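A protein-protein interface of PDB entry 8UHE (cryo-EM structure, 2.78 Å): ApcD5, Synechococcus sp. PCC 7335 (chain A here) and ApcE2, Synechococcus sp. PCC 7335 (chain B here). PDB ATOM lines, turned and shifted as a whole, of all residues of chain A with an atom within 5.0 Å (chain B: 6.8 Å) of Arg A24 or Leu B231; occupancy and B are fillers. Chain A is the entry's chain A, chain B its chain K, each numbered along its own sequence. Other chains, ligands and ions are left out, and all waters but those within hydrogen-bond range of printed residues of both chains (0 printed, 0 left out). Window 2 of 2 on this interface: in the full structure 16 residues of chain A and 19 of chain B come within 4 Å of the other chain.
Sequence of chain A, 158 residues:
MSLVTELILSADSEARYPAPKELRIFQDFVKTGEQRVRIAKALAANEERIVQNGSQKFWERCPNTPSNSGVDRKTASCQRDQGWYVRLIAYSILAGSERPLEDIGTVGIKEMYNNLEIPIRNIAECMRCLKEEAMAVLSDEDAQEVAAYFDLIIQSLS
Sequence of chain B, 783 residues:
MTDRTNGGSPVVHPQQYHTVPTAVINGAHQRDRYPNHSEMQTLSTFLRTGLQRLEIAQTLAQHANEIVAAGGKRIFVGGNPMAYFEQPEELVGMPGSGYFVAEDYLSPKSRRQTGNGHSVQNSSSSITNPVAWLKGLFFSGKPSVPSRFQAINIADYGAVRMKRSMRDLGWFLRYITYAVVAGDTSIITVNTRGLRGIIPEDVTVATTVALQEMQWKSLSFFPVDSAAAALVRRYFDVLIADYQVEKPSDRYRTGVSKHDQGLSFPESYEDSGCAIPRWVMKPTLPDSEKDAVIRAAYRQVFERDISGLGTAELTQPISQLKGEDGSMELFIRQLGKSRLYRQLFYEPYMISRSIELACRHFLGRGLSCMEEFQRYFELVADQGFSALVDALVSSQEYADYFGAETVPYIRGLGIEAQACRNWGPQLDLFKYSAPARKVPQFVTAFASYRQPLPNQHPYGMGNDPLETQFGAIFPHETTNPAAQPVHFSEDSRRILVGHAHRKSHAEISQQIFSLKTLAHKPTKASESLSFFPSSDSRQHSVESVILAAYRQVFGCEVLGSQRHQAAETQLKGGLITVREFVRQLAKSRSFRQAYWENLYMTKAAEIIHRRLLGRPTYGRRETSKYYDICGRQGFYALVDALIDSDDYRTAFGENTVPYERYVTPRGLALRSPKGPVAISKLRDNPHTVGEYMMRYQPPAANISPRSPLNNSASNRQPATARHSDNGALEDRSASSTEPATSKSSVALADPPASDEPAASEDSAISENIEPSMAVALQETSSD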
ATOM      1  N   PRO A  20      26.076  19.153  -8.026  1.00  0.00           N
ATOM      2  CA  PRO A  20      25.467  20.215  -7.209  1.00  0.00           C
ATOM      3  C   PRO A  20      24.744  19.719  -5.971  1.00  0.00           C
ATOM      4  O   PRO A  20      24.850  20.355  -4.921  1.00  0.00           O
ATOM      5  CB  PRO A  20      24.491  20.884  -8.184  1.00  0.00           C
ATOM      6  CG  PRO A  20      24.958  20.512  -9.560  1.00  0.00           C
ATOM      7  CD  PRO A  20      26.053  19.493  -9.459  1.00  0.00           C
ATOM      8  N   LYS A  21      24.048  18.583  -6.051  1.00  0.00           N
ATOM      9  CA  LYS A  21      23.372  18.033  -4.880  1.00  0.00           C
ATOM     10  C   LYS A  21      24.365  17.582  -3.808  1.00  0.00           C
ATOM     11  O   LYS A  21      24.124  17.781  -2.607  1.00  0.00           O
ATOM     12  CB  LYS A  21      22.461  16.889  -5.320  1.00  0.00           C
ATOM     13  CG  LYS A  21      23.131  15.860  -6.224  1.00  0.00           C
ATOM     14  CD  LYS A  21      22.109  15.060  -7.009  1.00  0.00           C
ATOM     15  CE  LYS A  21      22.678  13.722  -7.447  1.00  0.00           C
ATOM     16  NZ  LYS A  21      21.617  12.685  -7.522  1.00  0.00           N
ATOM     17  N   GLU A  22      25.494  16.992  -4.219  1.00  0.00           N
ATOM     18  CA  GLU A  22      26.539  16.614  -3.268  1.00  0.00           C
ATOM     19  C   GLU A  22      27.123  17.841  -2.576  1.00  0.00           C
ATOM     20  O   GLU A  22      27.419  17.817  -1.375  1.00  0.00           O
ATOM     21  CB  GLU A  22      27.640  15.825  -3.983  1.00  0.00           C
ATOM     22  CG  GLU A  22      27.161  14.587  -4.736  1.00  0.00           C
ATOM     23  CD  GLU A  22      26.904  13.404  -3.822  1.00  0.00           C
ATOM     24  OE1 GLU A  22      25.820  13.343  -3.206  1.00  0.00           O
ATOM     25  OE2 GLU A  22      27.798  12.539  -3.706  1.00  0.00           O
ATOM     26  N   LEU A  23      27.285  18.934  -3.316  1.00  0.00           N
ATOM     27  CA  LEU A  23      27.777  20.154  -2.691  1.00  0.00           C
ATOM     28  C   LEU A  23      26.708  20.849  -1.848  1.00  0.00           C
ATOM     29  O   LEU A  23      27.060  21.561  -0.900  1.00  0.00           O
ATOM     30  CB  LEU A  23      28.345  21.074  -3.773  1.00  0.00           C
ATOM     31  CG  LEU A  23      29.624  20.530  -4.437  1.00  0.00           C
ATOM     32  CD1 LEU A  23      30.425  21.649  -5.043  1.00  0.00           C
ATOM     33  CD2 LEU A  23      30.511  19.744  -3.468  1.00  0.00           C
ATOM     34  N   ARG A  24      25.424  20.625  -2.138  1.00  0.00           N
ATOM     35  CA  ARG A  24      24.350  21.024  -1.225  1.00  0.00           C
ATOM     36  C   ARG A  24      24.481  20.287   0.104  1.00  0.00           C
ATOM     37  O   ARG A  24      24.318  20.880   1.175  1.00  0.00           O
ATOM     38  CB  ARG A  24      22.977  20.742  -1.844  1.00  0.00           C
ATOM     39  CG  ARG A  24      22.231  21.957  -2.362  1.00  0.00           C
ATOM     40  CD  ARG A  24      22.408  22.054  -3.854  1.00  0.00           C
ATOM     41  NE  ARG A  24      21.359  22.805  -4.528  1.00  0.00           N
ATOM     42  CZ  ARG A  24      21.580  23.615  -5.554  1.00  0.00           C
ATOM     43  NH1 ARG A  24      22.797  23.796  -6.039  1.00  0.00           N
ATOM     44  NH2 ARG A  24      20.555  24.252  -6.110  1.00  0.00           N
ATOM     45  N   ILE A  25      24.754  18.981   0.032  1.00  0.00           N
ATOM     46  CA  ILE A  25      24.980  18.125   1.197  1.00  0.00           C
ATOM     47  C   ILE A  25      26.138  18.688   2.004  1.00  0.00           C
ATOM     48  O   ILE A  25      26.060  18.806   3.233  1.00  0.00           O
ATOM     49  CB  ILE A  25      25.299  16.684   0.765  1.00  0.00           C
ATOM     50  CG1 ILE A  25      24.042  15.941   0.373  1.00  0.00           C
ATOM     51  CG2 ILE A  25      26.000  15.909   1.867  1.00  0.00           C
ATOM     52  CD1 ILE A  25      24.325  15.075  -0.768  1.00  0.00           C
ATOM     53  N   PHE A  26      27.224  19.005   1.301  1.00  0.00           N
ATOM     54  CA  PHE A  26      28.413  19.632   1.861  1.00  0.00           C
ATOM     55  C   PHE A  26      28.093  20.887   2.659  1.00  0.00           C
ATOM     56  O   PHE A  26      28.392  20.975   3.856  1.00  0.00           O
ATOM     57  CB  PHE A  26      29.374  19.988   0.731  1.00  0.00           C
ATOM     58  CG  PHE A  26      30.795  19.659   1.018  1.00  0.00           C
ATOM     59  CD1 PHE A  26      31.697  20.658   1.302  1.00  0.00           C
ATOM     60  CD2 PHE A  26      31.235  18.374   0.994  1.00  0.00           C
ATOM     61  CE1 PHE A  26      33.008  20.358   1.571  1.00  0.00           C
ATOM     62  CE2 PHE A  26      32.503  18.070   1.233  1.00  0.00           C
ATOM     63  CZ  PHE A  26      33.410  19.061   1.538  1.00  0.00           C
ATOM     64  N   GLN A  27      27.436  21.840   2.001  1.00  0.00           N
ATOM     65  CA  GLN A  27      27.201  23.172   2.546  1.00  0.00           C
ATOM     66  C   GLN A  27      26.134  23.133   3.648  1.00  0.00           C
ATOM     67  O   GLN A  27      25.964  24.099   4.399  1.00  0.00           O
ATOM     68  CB  GLN A  27      26.862  24.102   1.364  1.00  0.00           C
ATOM     69  CG  GLN A  27      26.065  25.364   1.607  1.00  0.00           C
ATOM     70  CD  GLN A  27      25.895  26.192   0.353  1.00  0.00           C
ATOM     71  OE1 GLN A  27      26.752  26.178  -0.528  1.00  0.00           O
ATOM     72  NE2 GLN A  27      24.785  26.917   0.263  1.00  0.00           N
ATOM     73  N   ASP A  28      25.458  21.989   3.802  1.00  0.00           N
ATOM     74  CA  ASP A  28      24.426  21.813   4.822  1.00  0.00           C
ATOM     75  C   ASP A  28      24.962  21.082   6.045  1.00  0.00           C
ATOM     76  O   ASP A  28      24.652  21.448   7.184  1.00  0.00           O
ATOM     77  CB  ASP A  28      23.239  21.040   4.251  1.00  0.00           C
ATOM     78  CG  ASP A  28      22.065  21.932   3.941  1.00  0.00           C
ATOM     79  OD1 ASP A  28      22.256  23.165   3.921  1.00  0.00           O
ATOM     80  OD2 ASP A  28      20.955  21.405   3.720  1.00  0.00           O
ATOM     81  N   PHE A  29      25.745  20.029   5.812  1.00  0.00           N
ATOM     82  CA  PHE A  29      26.506  19.344   6.849  1.00  0.00           C
ATOM     83  C   PHE A  29      27.454  20.330   7.516  1.00  0.00           C
ATOM     84  O   PHE A  29      27.733  20.230   8.715  1.00  0.00           O
ATOM     85  CB  PHE A  29      27.267  18.168   6.234  1.00  0.00           C
ATOM     86  CG  PHE A  29      28.324  17.584   7.124  1.00  0.00           C
ATOM     87  CD1 PHE A  29      27.982  16.771   8.189  1.00  0.00           C
ATOM     88  CD2 PHE A  29      29.666  17.836   6.882  1.00  0.00           C
ATOM     89  CE1 PHE A  29      28.956  16.224   8.998  1.00  0.00           C
ATOM     90  CE2 PHE A  29      30.642  17.290   7.686  1.00  0.00           C
ATOM     91  CZ  PHE A  29      30.286  16.489   8.749  1.00  0.00           C
ATOM     92  N   GLN B  41      20.472  12.779   2.592  1.00  0.00           N
ATOM     93  CA  GLN B  41      20.450  14.219   2.557  1.00  0.00           C
ATOM     94  C   GLN B  41      20.295  14.726   1.136  1.00  0.00           C
ATOM     95  O   GLN B  41      19.667  15.764   0.936  1.00  0.00           O
ATOM     96  CB  GLN B  41      21.714  14.765   3.220  1.00  0.00           C
ATOM     97  CG  GLN B  41      21.492  15.130   4.687  1.00  0.00           C
ATOM     98  CD  GLN B  41      22.768  15.505   5.411  1.00  0.00           C
ATOM     99  OE1 GLN B  41      23.747  15.920   4.793  1.00  0.00           O
ATOM    100  NE2 GLN B  41      22.762  15.362   6.732  1.00  0.00           N
ATOM    101  N   THR B  45      17.111  16.987   0.713  1.00  0.00           N
ATOM    102  CA  THR B  45      17.380  18.370   0.328  1.00  0.00           C
ATOM    103  C   THR B  45      16.769  18.701  -1.026  1.00  0.00           C
ATOM    104  O   THR B  45      16.258  19.811  -1.226  1.00  0.00           O
ATOM    105  CB  THR B  45      18.887  18.634   0.309  1.00  0.00           C
ATOM    106  OG1 THR B  45      19.518  17.937   1.389  1.00  0.00           O
ATOM    107  CG2 THR B  45      19.170  20.121   0.437  1.00  0.00           C
ATOM    108  N   THR B  49      13.927  21.514  -1.797  1.00  0.00           N
ATOM    109  CA  THR B  49      13.918  22.530  -2.846  1.00  0.00           C
ATOM    110  C   THR B  49      12.794  22.327  -3.851  1.00  0.00           C
ATOM    111  O   THR B  49      12.568  23.225  -4.668  1.00  0.00           O
ATOM    112  CB  THR B  49      15.244  22.561  -3.608  1.00  0.00           C
ATOM    113  OG1 THR B  49      15.408  21.335  -4.330  1.00  0.00           O
ATOM    114  CG2 THR B  49      16.414  22.763  -2.657  1.00  0.00           C
ATOM    115  N   GLN B  52      10.507  25.291  -4.604  1.00  0.00           N
ATOM    116  CA  GLN B  52      11.055  26.318  -5.478  1.00  0.00           C
ATOM    117  C   GLN B  52      11.167  25.816  -6.908  1.00  0.00           C
ATOM    118  O   GLN B  52      10.887  26.556  -7.856  1.00  0.00           O
ATOM    119  CB  GLN B  52      12.412  26.774  -4.944  1.00  0.00           C
ATOM    120  CG  GLN B  52      12.384  27.103  -3.457  1.00  0.00           C
ATOM    121  CD  GLN B  52      13.597  26.583  -2.709  1.00  0.00           C
ATOM    122  OE1 GLN B  52      14.724  26.663  -3.197  1.00  0.00           O
ATOM    123  NE2 GLN B  52      13.367  26.035  -1.521  1.00  0.00           N
ATOM    124  N   ARG B  53      11.548  24.550  -7.081  1.00  0.00           N
ATOM    125  CA  ARG B  53      11.684  23.999  -8.428  1.00  0.00           C
ATOM    126  C   ARG B  53      10.339  23.915  -9.142  1.00  0.00           C
ATOM    127  O   ARG B  53      10.224  24.306 -10.314  1.00  0.00           O
ATOM    128  CB  ARG B  53      12.362  22.633  -8.362  1.00  0.00           C
ATOM    129  CG  ARG B  53      13.604  22.646  -7.506  1.00  0.00           C
ATOM    130  CD  ARG B  53      14.362  21.343  -7.512  1.00  0.00           C
ATOM    131  NE  ARG B  53      15.711  21.534  -6.993  1.00  0.00           N
ATOM    132  CZ  ARG B  53      16.721  22.038  -7.688  1.00  0.00           C
ATOM    133  NH1 ARG B  53      16.583  22.386  -8.956  1.00  0.00           N
ATOM    134  NH2 ARG B  53      17.900  22.200  -7.094  1.00  0.00           N
ATOM    135  N   ILE B  56       9.212  27.455 -10.056  1.00  0.00           N
ATOM    136  CA  ILE B  56       9.987  27.945 -11.198  1.00  0.00           C
ATOM    137  C   ILE B  56       9.433  27.376 -12.494  1.00  0.00           C
ATOM    138  O   ILE B  56       9.229  28.100 -13.479  1.00  0.00           O
ATOM    139  CB  ILE B  56      11.477  27.588 -11.044  1.00  0.00           C
ATOM    140  CG1 ILE B  56      12.163  28.473 -10.020  1.00  0.00           C
ATOM    141  CG2 ILE B  56      12.211  27.724 -12.365  1.00  0.00           C
ATOM    142  CD1 ILE B  56      13.421  27.857  -9.507  1.00  0.00           C
ATOM    143  N   VAL B 180      14.609  21.592 -14.166  1.00  0.00           N
ATOM    144  CA  VAL B 180      14.341  22.260 -12.894  1.00  0.00           C
ATOM    145  C   VAL B 180      13.498  21.367 -11.991  1.00  0.00           C
ATOM    146  O   VAL B 180      13.808  21.185 -10.808  1.00  0.00           O
ATOM    147  CB  VAL B 180      13.671  23.625 -13.137  1.00  0.00           C
ATOM    148  CG1 VAL B 180      13.064  24.156 -11.865  1.00  0.00           C
ATOM    149  CG2 VAL B 180      14.682  24.628 -13.669  1.00  0.00           C
ATOM    150  N   LEU B 219      15.006  35.477 -16.220  1.00  0.00           N
ATOM    151  CA  LEU B 219      15.419  36.121 -14.983  1.00  0.00           C
ATOM    152  C   LEU B 219      14.753  37.477 -14.800  1.00  0.00           C
ATOM    153  O   LEU B 219      14.629  37.950 -13.665  1.00  0.00           O
ATOM    154  CB  LEU B 219      16.935  36.246 -14.966  1.00  0.00           C
ATOM    155  CG  LEU B 219      17.488  34.825 -14.979  1.00  0.00           C
ATOM    156  CD1 LEU B 219      18.950  34.805 -15.149  1.00  0.00           C
ATOM    157  CD2 LEU B 219      17.089  34.108 -13.723  1.00  0.00           C
ATOM    158  N   PHE B 222      11.689  36.866 -12.937  1.00  0.00           N
ATOM    159  CA  PHE B 222      11.908  36.025 -11.762  1.00  0.00           C
ATOM    160  C   PHE B 222      12.961  36.721 -10.907  1.00  0.00           C
ATOM    161  O   PHE B 222      14.164  36.615 -11.198  1.00  0.00           O
ATOM    162  CB  PHE B 222      12.340  34.614 -12.153  1.00  0.00           C
ATOM    163  CG  PHE B 222      12.261  33.622 -11.030  1.00  0.00           C
ATOM    164  CD1 PHE B 222      11.035  33.161 -10.584  1.00  0.00           C
ATOM    165  CD2 PHE B 222      13.412  33.137 -10.435  1.00  0.00           C
ATOM    166  CE1 PHE B 222      10.956  32.246  -9.552  1.00  0.00           C
ATOM    167  CE2 PHE B 222      13.338  32.219  -9.404  1.00  0.00           C
ATOM    168  CZ  PHE B 222      12.110  31.780  -8.958  1.00  0.00           C
ATOM    169  N   ALA B 227      17.282  35.037  -4.697  1.00  0.00           N
ATOM    170  CA  ALA B 227      16.334  33.939  -4.811  1.00  0.00           C
ATOM    171  C   ALA B 227      16.891  32.873  -5.751  1.00  0.00           C
ATOM    172  O   ALA B 227      18.073  32.867  -6.107  1.00  0.00           O
ATOM    173  CB  ALA B 227      14.979  34.457  -5.285  1.00  0.00           C
ATOM    174  N   ALA B 228      16.024  31.960  -6.174  1.00  0.00           N
ATOM    175  CA  ALA B 228      16.293  30.905  -7.146  1.00  0.00           C
ATOM    176  C   ALA B 228      16.499  31.429  -8.576  1.00  0.00           C
ATOM    177  O   ALA B 228      16.599  30.658  -9.546  1.00  0.00           O
ATOM    178  CB  ALA B 228      15.155  29.891  -7.113  1.00  0.00           C
ATOM    179  N   ALA B 229      16.547  32.730  -8.770  1.00  0.00           N
ATOM    180  CA  ALA B 229      17.000  33.228 -10.036  1.00  0.00           C
ATOM    181  C   ALA B 229      18.478  32.961 -10.272  1.00  0.00           C
ATOM    182  O   ALA B 229      18.909  32.842 -11.422  1.00  0.00           O
ATOM    183  CB  ALA B 229      16.672  34.658 -10.002  1.00  0.00           C
ATOM    184  N   ALA B 230      19.248  32.779  -9.200  1.00  0.00           N
ATOM    185  CA  ALA B 230      20.584  32.213  -9.341  1.00  0.00           C
ATOM    186  C   ALA B 230      20.522  30.792  -9.895  1.00  0.00           C
ATOM    187  O   ALA B 230      21.347  30.411 -10.733  1.00  0.00           O
ATOM    188  CB  ALA B 230      21.309  32.238  -7.996  1.00  0.00           C
ATOM    189  N   LEU B 231      19.539  30.000  -9.452  1.00  0.00           N
ATOM    190  CA  LEU B 231      19.368  28.644  -9.971  1.00  0.00           C
ATOM    191  C   LEU B 231      18.981  28.649 -11.448  1.00  0.00           C
ATOM    192  O   LEU B 231      19.506  27.856 -12.241  1.00  0.00           O
ATOM    193  CB  LEU B 231      18.311  27.904  -9.152  1.00  0.00           C
ATOM    194  CG  LEU B 231      17.950  26.486  -9.597  1.00  0.00           C
ATOM    195  CD1 LEU B 231      19.054  25.524  -9.233  1.00  0.00           C
ATOM    196  CD2 LEU B 231      16.636  26.041  -8.989  1.00  0.00           C
ATOM    197  N   VAL B 232      18.054  29.532 -11.830  1.00  0.00           N
ATOM    198  CA  VAL B 232      17.630  29.619 -13.230  1.00  0.00           C
ATOM    199  C   VAL B 232      18.775  30.128 -14.104  1.00  0.00           C
ATOM    200  O   VAL B 232      18.977  29.650 -15.230  1.00  0.00           O
ATOM    201  CB  VAL B 232      16.368  30.496 -13.351  1.00  0.00           C
ATOM    202  CG1 VAL B 232      15.979  30.711 -14.810  1.00  0.00           C
ATOM    203  CG2 VAL B 232      15.220  29.860 -12.596  1.00  0.00           C
ATOM    204  N   ARG B 233      19.560  31.082 -13.586  1.00  0.00           N
ATOM    205  CA  ARG B 233      20.765  31.532 -14.278  1.00  0.00           C
ATOM    206  C   ARG B 233      21.761  30.394 -14.458  1.00  0.00           C
ATOM    207  O   ARG B 233      22.341  30.241 -15.538  1.00  0.00           O
ATOM    208  CB  ARG B 233      21.408  32.689 -13.508  1.00  0.00           C
ATOM    209  CG  ARG B 233      22.843  33.004 -13.912  1.00  0.00           C
ATOM    210  CD  ARG B 233      23.134  34.502 -14.036  1.00  0.00           C
ATOM    211  NE  ARG B 233      22.209  35.229 -14.899  1.00  0.00           N
ATOM    212  CZ  ARG B 233      21.893  36.510 -14.745  1.00  0.00           C
ATOM    213  NH1 ARG B 233      22.364  37.220 -13.736  1.00  0.00           N
ATOM    214  NH2 ARG B 233      21.094  37.098 -15.632  1.00  0.00           N
ATOM    215  N   ARG B 234      21.959  29.574 -13.420  1.00  0.00           N
ATOM    216  CA  ARG B 234      22.899  28.461 -13.519  1.00  0.00           C
ATOM    217  C   ARG B 234      22.430  27.425 -14.535  1.00  0.00           C
ATOM    218  O   ARG B 234      23.234  26.900 -15.312  1.00  0.00           O
ATOM    219  CB  ARG B 234      23.097  27.812 -12.148  1.00  0.00           C
ATOM    220  CG  ARG B 234      23.713  26.424 -12.217  1.00  0.00           C
ATOM    221  CD  ARG B 234      24.083  25.877 -10.860  1.00  0.00           C
ATOM    222  NE  ARG B 234      23.658  24.489 -10.751  1.00  0.00           N
ATOM    223  CZ  ARG B 234      22.795  24.040  -9.851  1.00  0.00           C
ATOM    224  NH1 ARG B 234      22.299  24.831  -8.914  1.00  0.00           N
ATOM    225  NH2 ARG B 234      22.415  22.767  -9.898  1.00  0.00           N
ATOM    226  N   TYR B 235      21.129  27.131 -14.559  1.00  0.00           N
ATOM    227  CA  TYR B 235      20.628  26.114 -15.480  1.00  0.00           C
ATOM    228  C   TYR B 235      20.667  26.603 -16.925  1.00  0.00           C
ATOM    229  O   TYR B 235      21.024  25.842 -17.835  1.00  0.00           O
ATOM    230  CB  TYR B 235      19.217  25.694 -15.076  1.00  0.00           C
ATOM    231  CG  TYR B 235      19.197  24.571 -14.060  1.00  0.00           C
ATOM    232  CD1 TYR B 235      20.062  24.573 -12.973  1.00  0.00           C
ATOM    233  CD2 TYR B 235      18.316  23.507 -14.193  1.00  0.00           C
ATOM    234  CE1 TYR B 235      20.049  23.551 -12.049  1.00  0.00           C
ATOM    235  CE2 TYR B 235      18.296  22.480 -13.270  1.00  0.00           C
ATOM    236  CZ  TYR B 235      19.164  22.508 -12.201  1.00  0.00           C
ATOM    237  OH  TYR B 235      19.146  21.487 -11.281  1.00  0.00           O
ATOM    238  N   PHE B 236      20.336  27.880 -17.153  1.00  0.00           N
ATOM    239  CA  PHE B 236      20.495  28.459 -18.484  1.00  0.00           C
ATOM    240  C   PHE B 236      21.964  28.508 -18.896  1.00  0.00           C
ATOM    241  O   PHE B 236      22.296  28.276 -20.065  1.00  0.00           O
ATOM    242  CB  PHE B 236      19.881  29.858 -18.520  1.00  0.00           C
ATOM    243  CG  PHE B 236      18.485  29.907 -19.082  1.00  0.00           C
ATOM    244  CD1 PHE B 236      18.275  30.034 -20.447  1.00  0.00           C
ATOM    245  CD2 PHE B 236      17.385  29.843 -18.243  1.00  0.00           C
ATOM    246  CE1 PHE B 236      16.995  30.097 -20.965  1.00  0.00           C
ATOM    247  CE2 PHE B 236      16.101  29.898 -18.755  1.00  0.00           C
ATOM    248  CZ  PHE B 236      15.904  30.027 -20.117  1.00  0.00           C
ATOM    249  N   ASP B 237      22.858  28.810 -17.948  1.00  0.00           N
ATOM    250  CA  ASP B 237      24.291  28.829 -18.233  1.00  0.00           C
ATOM    251  C   ASP B 237      24.806  27.441 -18.583  1.00  0.00           C
ATOM    252  O   ASP B 237      25.670  27.294 -19.452  1.00  0.00           O
ATOM    253  CB  ASP B 237      25.055  29.383 -17.032  1.00  0.00           C
ATOM    254  CG  ASP B 237      25.436  30.836 -17.203  1.00  0.00           C
ATOM    255  OD1 ASP B 237      25.511  31.300 -18.360  1.00  0.00           O
ATOM    256  OD2 ASP B 237      25.668  31.510 -16.179  1.00  0.00           O
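The side-chain hydroxyl of Thr B49 is in hydrogen-bond range of the guanidinium group of Arg B53.
Printed residues of chain B within 4 Å of Pro A20: Arg B234 (3.3 Å).
Arg A24 touches three residues of chain B.
Printed residues of chain B within 4 Å of Ile A25: Gln B41 (3.7 Å).
Phe A26 touches none of the printed residues of chain B.
Printed residues of chain A within 4 Å of Thr B45: Asp A28 (3.95 Å).
Ala B227 touches none of the printed residues of chain A.
Leu B231 touches just one residue of chain A: Arg A24 (3.7 Å).
The nearest residue of chain B that does not touch Arg A24 is Thr B45 (4.5 Å).
The nearest printed residue of chain A that does not touch Leu B231 is Pro A20 (7.2 Å).
The guanidinium group of Arg A24 lies close to the guanidinium group of Arg B53.
The guanidinium group (NH1) of Arg A24 lies close to the guanidinium group (NH1) of Arg B234 (3.1 Å).
Of the 10 printed residues of chain A, 4 touch a printed residue of chain B.
Printed residues of chain A that touch a printed residue of chain B: Pro A20, Arg A24, Ile A25 and Asp A28.
Of the 20 printed residues of chain B, 5 touch a printed residue of chain A.
Printed residues of chain B that touch a printed residue of chain A: Gln B41, Thr B45, Arg B53, Leu B231 and Arg B234.
Hydrophobic or aromatic side chains of chain B that line the printed part of chain A: Leu B231.
Along chain B the printed residues that touch a printed residue of chain A span positions 41 to 234.
Among the printed residues, 6 pairs touch across the chains.
Among the printed residues, merely in contact across the chains: Pro A20 with Arg B234, Arg A24 with Leu B231, Ile A25 with Gln B41 and Asp A28 with Thr B45.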
